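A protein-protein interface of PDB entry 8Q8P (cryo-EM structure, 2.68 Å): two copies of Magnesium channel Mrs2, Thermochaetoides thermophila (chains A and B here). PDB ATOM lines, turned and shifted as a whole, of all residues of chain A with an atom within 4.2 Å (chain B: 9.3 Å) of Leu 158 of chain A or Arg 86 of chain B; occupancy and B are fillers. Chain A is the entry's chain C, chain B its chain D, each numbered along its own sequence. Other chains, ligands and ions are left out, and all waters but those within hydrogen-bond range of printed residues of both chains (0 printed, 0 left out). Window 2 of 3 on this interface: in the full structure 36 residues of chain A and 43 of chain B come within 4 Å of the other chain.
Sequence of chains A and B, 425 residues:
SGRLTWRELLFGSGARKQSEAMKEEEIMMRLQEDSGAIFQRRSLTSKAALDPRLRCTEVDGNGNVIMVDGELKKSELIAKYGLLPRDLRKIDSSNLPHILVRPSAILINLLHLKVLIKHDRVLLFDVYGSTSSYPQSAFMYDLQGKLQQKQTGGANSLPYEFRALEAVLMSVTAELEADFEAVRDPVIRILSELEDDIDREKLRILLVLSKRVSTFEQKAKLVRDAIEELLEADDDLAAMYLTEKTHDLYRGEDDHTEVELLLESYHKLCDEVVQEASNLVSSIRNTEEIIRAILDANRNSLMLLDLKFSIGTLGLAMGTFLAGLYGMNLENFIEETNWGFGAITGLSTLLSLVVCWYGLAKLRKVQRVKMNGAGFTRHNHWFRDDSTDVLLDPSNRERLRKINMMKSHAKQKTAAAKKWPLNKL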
ATOM      1  N   ASN A 156     -19.870   7.942 -24.925  1.00  0.00           N
ATOM      2  CA  ASN A 156     -20.173   6.595 -24.452  1.00  0.00           C
ATOM      3  C   ASN A 156     -18.924   5.769 -24.171  1.00  0.00           C
ATOM      4  O   ASN A 156     -18.955   4.539 -24.313  1.00  0.00           O
ATOM      5  CB  ASN A 156     -21.070   5.877 -25.462  1.00  0.00           C
ATOM      6  CG  ASN A 156     -22.431   6.532 -25.601  1.00  0.00           C
ATOM      7  OD1 ASN A 156     -22.938   7.141 -24.658  1.00  0.00           O
ATOM      8  ND2 ASN A 156     -23.030   6.408 -26.778  1.00  0.00           N
ATOM      9  N   SER A 157     -17.825   6.407 -23.775  1.00  0.00           N
ATOM     10  CA  SER A 157     -16.612   5.679 -23.431  1.00  0.00           C
ATOM     11  C   SER A 157     -16.701   5.150 -22.007  1.00  0.00           C
ATOM     12  O   SER A 157     -17.157   5.846 -21.096  1.00  0.00           O
ATOM     13  CB  SER A 157     -15.388   6.580 -23.583  1.00  0.00           C
ATOM     14  OG  SER A 157     -14.195   5.877 -23.280  1.00  0.00           O
ATOM     15  N   LEU A 158     -16.258   3.907 -21.817  1.00  0.00           N
ATOM     16  CA  LEU A 158     -16.325   3.265 -20.517  1.00  0.00           C
ATOM     17  C   LEU A 158     -14.929   2.900 -20.022  1.00  0.00           C
ATOM     18  O   LEU A 158     -14.045   2.577 -20.822  1.00  0.00           O
ATOM     19  CB  LEU A 158     -17.192   2.000 -20.568  1.00  0.00           C
ATOM     20  CG  LEU A 158     -18.683   2.217 -20.830  1.00  0.00           C
ATOM     21  CD1 LEU A 158     -19.426   0.891 -20.829  1.00  0.00           C
ATOM     22  CD2 LEU A 158     -19.275   3.168 -19.802  1.00  0.00           C
ATOM     23  N   PRO A 159     -14.703   2.947 -18.716  1.00  0.00           N
ATOM     24  CA  PRO A 159     -13.388   2.614 -18.160  1.00  0.00           C
ATOM     25  C   PRO A 159     -13.161   1.105 -18.120  1.00  0.00           C
ATOM     26  O   PRO A 159     -13.963   0.310 -18.603  1.00  0.00           O
ATOM     27  CB  PRO A 159     -13.442   3.207 -16.745  1.00  0.00           C
ATOM     28  CG  PRO A 159     -14.608   4.150 -16.749  1.00  0.00           C
ATOM     29  CD  PRO A 159     -15.582   3.560 -17.711  1.00  0.00           C
ATOM     30  N   ARG A 163     -16.014  -1.972 -18.235  1.00  0.00           N
ATOM     31  CA  ARG A 163     -15.937  -2.895 -19.363  1.00  0.00           C
ATOM     32  C   ARG A 163     -15.797  -4.339 -18.900  1.00  0.00           C
ATOM     33  O   ARG A 163     -16.289  -5.252 -19.572  1.00  0.00           O
ATOM     34  CB  ARG A 163     -14.772  -2.521 -20.279  1.00  0.00           C
ATOM     35  CG  ARG A 163     -15.040  -1.314 -21.164  1.00  0.00           C
ATOM     36  CD  ARG A 163     -14.055  -1.250 -22.319  1.00  0.00           C
ATOM     37  NE  ARG A 163     -12.675  -1.129 -21.863  1.00  0.00           N
ATOM     38  CZ  ARG A 163     -12.013   0.016 -21.774  1.00  0.00           C
ATOM     39  NH1 ARG A 163     -12.576   1.167 -22.105  1.00  0.00           N
ATOM     40  NH2 ARG A 163     -10.755   0.007 -21.344  1.00  0.00           N
ATOM     41  N   GLU A 166     -19.382  -5.341 -17.423  1.00  0.00           N
ATOM     42  CA  GLU A 166     -20.350  -5.582 -18.488  1.00  0.00           C
ATOM     43  C   GLU A 166     -20.194  -6.984 -19.064  1.00  0.00           C
ATOM     44  O   GLU A 166     -21.187  -7.692 -19.274  1.00  0.00           O
ATOM     45  CB  GLU A 166     -20.191  -4.526 -19.580  1.00  0.00           C
ATOM     46  CG  GLU A 166     -21.240  -4.591 -20.670  1.00  0.00           C
ATOM     47  CD  GLU A 166     -21.103  -3.467 -21.675  1.00  0.00           C
ATOM     48  OE1 GLU A 166     -20.097  -2.731 -21.609  1.00  0.00           O
ATOM     49  OE2 GLU A 166     -22.003  -3.317 -22.528  1.00  0.00           O
ATOM     50  N   LEU A 261     -27.381   2.757 -15.174  1.00  0.00           N
ATOM     51  CA  LEU A 261     -27.908   2.356 -16.474  1.00  0.00           C
ATOM     52  C   LEU A 261     -27.331   1.018 -16.914  1.00  0.00           C
ATOM     53  O   LEU A 261     -28.023   0.214 -17.550  1.00  0.00           O
ATOM     54  CB  LEU A 261     -27.618   3.436 -17.518  1.00  0.00           C
ATOM     55  CG  LEU A 261     -28.686   4.506 -17.756  1.00  0.00           C
ATOM     56  CD1 LEU A 261     -29.004   5.276 -16.484  1.00  0.00           C
ATOM     57  CD2 LEU A 261     -28.252   5.455 -18.864  1.00  0.00           C
ATOM     58  N   LEU A 262     -26.060   0.766 -16.592  1.00  0.00           N
ATOM     59  CA  LEU A 262     -25.456  -0.518 -16.930  1.00  0.00           C
ATOM     60  C   LEU A 262     -26.137  -1.663 -16.188  1.00  0.00           C
ATOM     61  O   LEU A 262     -26.403  -2.720 -16.771  1.00  0.00           O
ATOM     62  CB  LEU A 262     -23.957  -0.481 -16.620  1.00  0.00           C
ATOM     63  CG  LEU A 262     -23.014  -1.471 -17.314  1.00  0.00           C
ATOM     64  CD1 LEU A 262     -21.602  -0.910 -17.336  1.00  0.00           C
ATOM     65  CD2 LEU A 262     -23.027  -2.829 -16.631  1.00  0.00           C
ATOM     66  N   ILE B  78     -28.851   4.469 -32.669  1.00  0.00           N
ATOM     67  CA  ILE B  78     -27.778   5.042 -31.864  1.00  0.00           C
ATOM     68  C   ILE B  78     -27.294   6.351 -32.472  1.00  0.00           C
ATOM     69  O   ILE B  78     -26.906   7.275 -31.747  1.00  0.00           O
ATOM     70  CB  ILE B  78     -26.627   4.032 -31.713  1.00  0.00           C
ATOM     71  CG1 ILE B  78     -27.168   2.661 -31.312  1.00  0.00           C
ATOM     72  CG2 ILE B  78     -25.616   4.522 -30.688  1.00  0.00           C
ATOM     73  CD1 ILE B  78     -26.104   1.593 -31.236  1.00  0.00           C
ATOM     74  N   LEU B  83     -30.121   6.754 -28.253  1.00  0.00           N
ATOM     75  CA  LEU B  83     -30.140   5.461 -27.588  1.00  0.00           C
ATOM     76  C   LEU B  83     -28.718   4.969 -27.327  1.00  0.00           C
ATOM     77  O   LEU B  83     -27.737   5.498 -27.854  1.00  0.00           O
ATOM     78  CB  LEU B  83     -30.916   4.440 -28.421  1.00  0.00           C
ATOM     79  CG  LEU B  83     -32.429   4.640 -28.502  1.00  0.00           C
ATOM     80  CD1 LEU B  83     -33.072   3.534 -29.322  1.00  0.00           C
ATOM     81  CD2 LEU B  83     -33.037   4.700 -27.110  1.00  0.00           C
ATOM     82  N   LEU B  84     -28.617   3.930 -26.491  1.00  0.00           N
ATOM     83  CA  LEU B  84     -27.355   3.314 -26.123  1.00  0.00           C
ATOM     84  C   LEU B  84     -27.182   1.978 -26.836  1.00  0.00           C
ATOM     85  O   LEU B  84     -28.167   1.315 -27.173  1.00  0.00           O
ATOM     86  CB  LEU B  84     -27.279   3.097 -24.609  1.00  0.00           C
ATOM     87  CG  LEU B  84     -27.245   4.359 -23.745  1.00  0.00           C
ATOM     88  CD1 LEU B  84     -27.118   4.000 -22.273  1.00  0.00           C
ATOM     89  CD2 LEU B  84     -26.111   5.276 -24.176  1.00  0.00           C
ATOM     90  N   PRO B  85     -25.936   1.565 -27.090  1.00  0.00           N
ATOM     91  CA  PRO B  85     -25.715   0.288 -27.789  1.00  0.00           C
ATOM     92  C   PRO B  85     -26.262  -0.923 -27.054  1.00  0.00           C
ATOM     93  O   PRO B  85     -26.584  -1.925 -27.704  1.00  0.00           O
ATOM     94  CB  PRO B  85     -24.186   0.220 -27.917  1.00  0.00           C
ATOM     95  CG  PRO B  85     -23.735   1.639 -27.830  1.00  0.00           C
ATOM     96  CD  PRO B  85     -24.680   2.302 -26.875  1.00  0.00           C
ATOM     97  N   ARG B  86     -26.381  -0.870 -25.728  1.00  0.00           N
ATOM     98  CA  ARG B  86     -26.864  -2.008 -24.959  1.00  0.00           C
ATOM     99  C   ARG B  86     -28.383  -2.117 -24.937  1.00  0.00           C
ATOM    100  O   ARG B  86     -28.906  -3.150 -24.502  1.00  0.00           O
ATOM    101  CB  ARG B  86     -26.341  -1.938 -23.520  1.00  0.00           C
ATOM    102  CG  ARG B  86     -26.862  -0.754 -22.721  1.00  0.00           C
ATOM    103  CD  ARG B  86     -26.484  -0.866 -21.252  1.00  0.00           C
ATOM    104  NE  ARG B  86     -25.039  -0.853 -21.055  1.00  0.00           N
ATOM    105  CZ  ARG B  86     -24.333   0.231 -20.766  1.00  0.00           C
ATOM    106  NH1 ARG B  86     -24.907   1.415 -20.628  1.00  0.00           N
ATOM    107  NH2 ARG B  86     -23.016   0.125 -20.610  1.00  0.00           N
ATOM    108  N   ASP B  87     -29.101  -1.089 -25.390  1.00  0.00           N
ATOM    109  CA  ASP B  87     -30.558  -1.129 -25.393  1.00  0.00           C
ATOM    110  C   ASP B  87     -31.128  -1.819 -26.626  1.00  0.00           C
ATOM    111  O   ASP B  87     -32.299  -2.218 -26.606  1.00  0.00           O
ATOM    112  CB  ASP B  87     -31.124   0.289 -25.296  1.00  0.00           C
ATOM    113  CG  ASP B  87     -30.672   1.012 -24.043  1.00  0.00           C
ATOM    114  OD1 ASP B  87     -30.479   0.345 -23.005  1.00  0.00           O
ATOM    115  OD2 ASP B  87     -30.509   2.249 -24.096  1.00  0.00           O
ATOM    116  N   LEU B  88     -30.328  -1.979 -27.684  1.00  0.00           N
ATOM    117  CA  LEU B  88     -30.844  -2.534 -28.932  1.00  0.00           C
ATOM    118  C   LEU B  88     -31.378  -3.947 -28.737  1.00  0.00           C
ATOM    119  O   LEU B  88     -32.400  -4.318 -29.325  1.00  0.00           O
ATOM    120  CB  LEU B  88     -29.755  -2.518 -30.004  1.00  0.00           C
ATOM    121  CG  LEU B  88     -29.269  -1.145 -30.471  1.00  0.00           C
ATOM    122  CD1 LEU B  88     -28.316  -1.293 -31.646  1.00  0.00           C
ATOM    123  CD2 LEU B  88     -30.442  -0.251 -30.838  1.00  0.00           C
ATOM    124  N   ARG B  89     -30.702  -4.751 -27.912  1.00  0.00           N
ATOM    125  CA  ARG B  89     -31.167  -6.110 -27.661  1.00  0.00           C
ATOM    126  C   ARG B  89     -32.530  -6.138 -26.979  1.00  0.00           C
ATOM    127  O   ARG B  89     -33.233  -7.150 -27.070  1.00  0.00           O
ATOM    128  CB  ARG B  89     -30.144  -6.877 -26.824  1.00  0.00           C
ATOM    129  CG  ARG B  89     -30.025  -6.410 -25.384  1.00  0.00           C
ATOM    130  CD  ARG B  89     -29.088  -7.314 -24.602  1.00  0.00           C
ATOM    131  NE  ARG B  89     -29.477  -8.715 -24.708  1.00  0.00           N
ATOM    132  CZ  ARG B  89     -28.781  -9.727 -24.207  1.00  0.00           C
ATOM    133  NH1 ARG B  89     -27.647  -9.530 -23.554  1.00  0.00           N
ATOM    134  NH2 ARG B  89     -29.235 -10.966 -24.366  1.00  0.00           N
ATOM    135  N   LYS B  90     -32.917  -5.056 -26.297  1.00  0.00           N
ATOM    136  CA  LYS B  90     -34.267  -4.985 -25.750  1.00  0.00           C
ATOM    137  C   LYS B  90     -35.296  -4.720 -26.842  1.00  0.00           C
ATOM    138  O   LYS B  90     -36.442  -5.171 -26.736  1.00  0.00           O
ATOM    139  CB  LYS B  90     -34.345  -3.904 -24.671  1.00  0.00           C
ATOM    140  CG  LYS B  90     -33.784  -4.330 -23.323  1.00  0.00           C
ATOM    141  CD  LYS B  90     -34.598  -5.469 -22.729  1.00  0.00           C
ATOM    142  CE  LYS B  90     -34.096  -5.849 -21.346  1.00  0.00           C
ATOM    143  NZ  LYS B  90     -34.914  -6.938 -20.740  1.00  0.00           N
ATOM    144  N   ILE B  91     -34.908  -3.992 -27.889  1.00  0.00           N
ATOM    145  CA  ILE B  91     -35.827  -3.700 -28.983  1.00  0.00           C
ATOM    146  C   ILE B  91     -36.069  -4.939 -29.837  1.00  0.00           C
ATOM    147  O   ILE B  91     -37.178  -5.154 -30.338  1.00  0.00           O
ATOM    148  CB  ILE B  91     -35.286  -2.528 -29.821  1.00  0.00           C
ATOM    149  CG1 ILE B  91     -35.071  -1.297 -28.938  1.00  0.00           C
ATOM    150  CG2 ILE B  91     -36.228  -2.201 -30.967  1.00  0.00           C
ATOM    151  CD1 ILE B  91     -34.510  -0.104 -29.683  1.00  0.00           C
ATOM    152  N   ASP B  92     -35.041  -5.773 -30.012  1.00  0.00           N
ATOM    153  CA  ASP B  92     -35.141  -6.905 -30.929  1.00  0.00           C
ATOM    154  C   ASP B  92     -36.160  -7.930 -30.443  1.00  0.00           C
ATOM    155  O   ASP B  92     -37.149  -8.214 -31.129  1.00  0.00           O
ATOM    156  CB  ASP B  92     -33.767  -7.553 -31.107  1.00  0.00           C
ATOM    157  CG  ASP B  92     -32.742  -6.594 -31.678  1.00  0.00           C
ATOM    158  OD1 ASP B  92     -33.098  -5.424 -31.929  1.00  0.00           O
ATOM    159  OD2 ASP B  92     -31.581  -7.009 -31.876  1.00  0.00           O
ATOM    160  N   SER B  94     -38.020  -8.959 -26.704  1.00  0.00           N
ATOM    161  CA  SER B  94     -38.240  -8.852 -25.268  1.00  0.00           C
ATOM    162  C   SER B  94     -39.738  -8.866 -25.009  1.00  0.00           C
ATOM    163  O   SER B  94     -40.482  -8.109 -25.639  1.00  0.00           O
ATOM    164  CB  SER B  94     -37.608  -7.577 -24.698  1.00  0.00           C
ATOM    165  OG  SER B  94     -36.195  -7.617 -24.795  1.00  0.00           O
ATOM    166  N   LEU B 100     -38.559   3.254 -20.806  1.00  0.00           N
ATOM    167  CA  LEU B 100     -37.235   3.807 -20.570  1.00  0.00           C
ATOM    168  C   LEU B 100     -37.216   5.278 -20.962  1.00  0.00           C
ATOM    169  O   LEU B 100     -37.697   5.651 -22.037  1.00  0.00           O
ATOM    170  CB  LEU B 100     -36.171   3.043 -21.364  1.00  0.00           C
ATOM    171  CG  LEU B 100     -36.083   1.539 -21.110  1.00  0.00           C
ATOM    172  CD1 LEU B 100     -34.979   0.921 -21.951  1.00  0.00           C
ATOM    173  CD2 LEU B 100     -35.859   1.256 -19.633  1.00  0.00           C
ATOM    174  N   ARG B 102     -34.919   8.479 -21.776  1.00  0.00           N
ATOM    175  CA  ARG B 102     -33.623   8.938 -22.242  1.00  0.00           C
ATOM    176  C   ARG B 102     -33.577  10.461 -22.260  1.00  0.00           C
ATOM    177  O   ARG B 102     -34.613  11.128 -22.177  1.00  0.00           O
ATOM    178  CB  ARG B 102     -33.341   8.377 -23.641  1.00  0.00           C
ATOM    179  CG  ARG B 102     -32.981   6.901 -23.643  1.00  0.00           C
ATOM    180  CD  ARG B 102     -31.688   6.657 -22.885  1.00  0.00           C
ATOM    181  NE  ARG B 102     -31.433   5.237 -22.675  1.00  0.00           N
ATOM    182  CZ  ARG B 102     -31.752   4.573 -21.572  1.00  0.00           C
ATOM    183  NH1 ARG B 102     -32.337   5.174 -20.549  1.00  0.00           N
ATOM    184  NH2 ARG B 102     -31.476   3.275 -21.494  1.00  0.00           N
ATOM    185  N   LEU B 107     -38.630   5.277 -24.779  1.00  0.00           N
ATOM    186  CA  LEU B 107     -38.801   3.949 -25.356  1.00  0.00           C
ATOM    187  C   LEU B 107     -39.901   3.224 -24.592  1.00  0.00           C
ATOM    188  O   LEU B 107     -39.849   3.136 -23.362  1.00  0.00           O
ATOM    189  CB  LEU B 107     -37.493   3.160 -25.307  1.00  0.00           C
ATOM    190  CG  LEU B 107     -37.505   1.764 -25.930  1.00  0.00           C
ATOM    191  CD1 LEU B 107     -37.891   1.844 -27.394  1.00  0.00           C
ATOM    192  CD2 LEU B 107     -36.150   1.095 -25.769  1.00  0.00           C
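CD2 of Leu 84 of chain B touches OD1 of Asn 156 of chain A, 3.7 Å away. Arg 86 of chain B touches Leu 158 of chain A (NH2 to CD1, 3.7 Å). CD1 of Leu 84 of chain B touches CD2 of Leu 261 of chain A, at 3.9 Å. Leu 262 of chain A touches Arg 86 of chain B.
No residue of chain B comes within 4 Å of Ser 157 of chain A. Of the printed residues of chain B, Leu 261 of chain A touches Leu 84. Of the printed residues of chain A, Leu 84 of chain B touches Asn 156 (3.7 Å) and Leu 261 (3.9 Å). Printed residues of chain B within 4 Å of Asn 156 of chain A: Leu 84. The nearest printed residue of chain B that does not touch Leu 261 of chain A is Arg 86 of chain B (4.2 Å).
O of Leu 158 of chain A is in hydrogen-bond range of NH1 of Arg 163 of chain A (2.4 Å). OD2 of Asp 87 of chain B sits close to N of Leu 84 of chain B, 3.5 Å away.
Of the 8 printed residues of chain A, 4 touch a printed residue of chain B. Hydrophobic or aromatic side chains of chain A that line the printed part of chain B: Leu 158, Leu 261 and Leu 262. Along chain B the printed residues that touch a printed residue of chain A span positions 84 to 86. Among the printed residues, 4 pairs touch across the chains. Among the printed residues, no Asp or Glu carboxylate lies within 4 Å of a Lys or Arg side-chain nitrogen of the other chain.
No position is printed for both chains.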
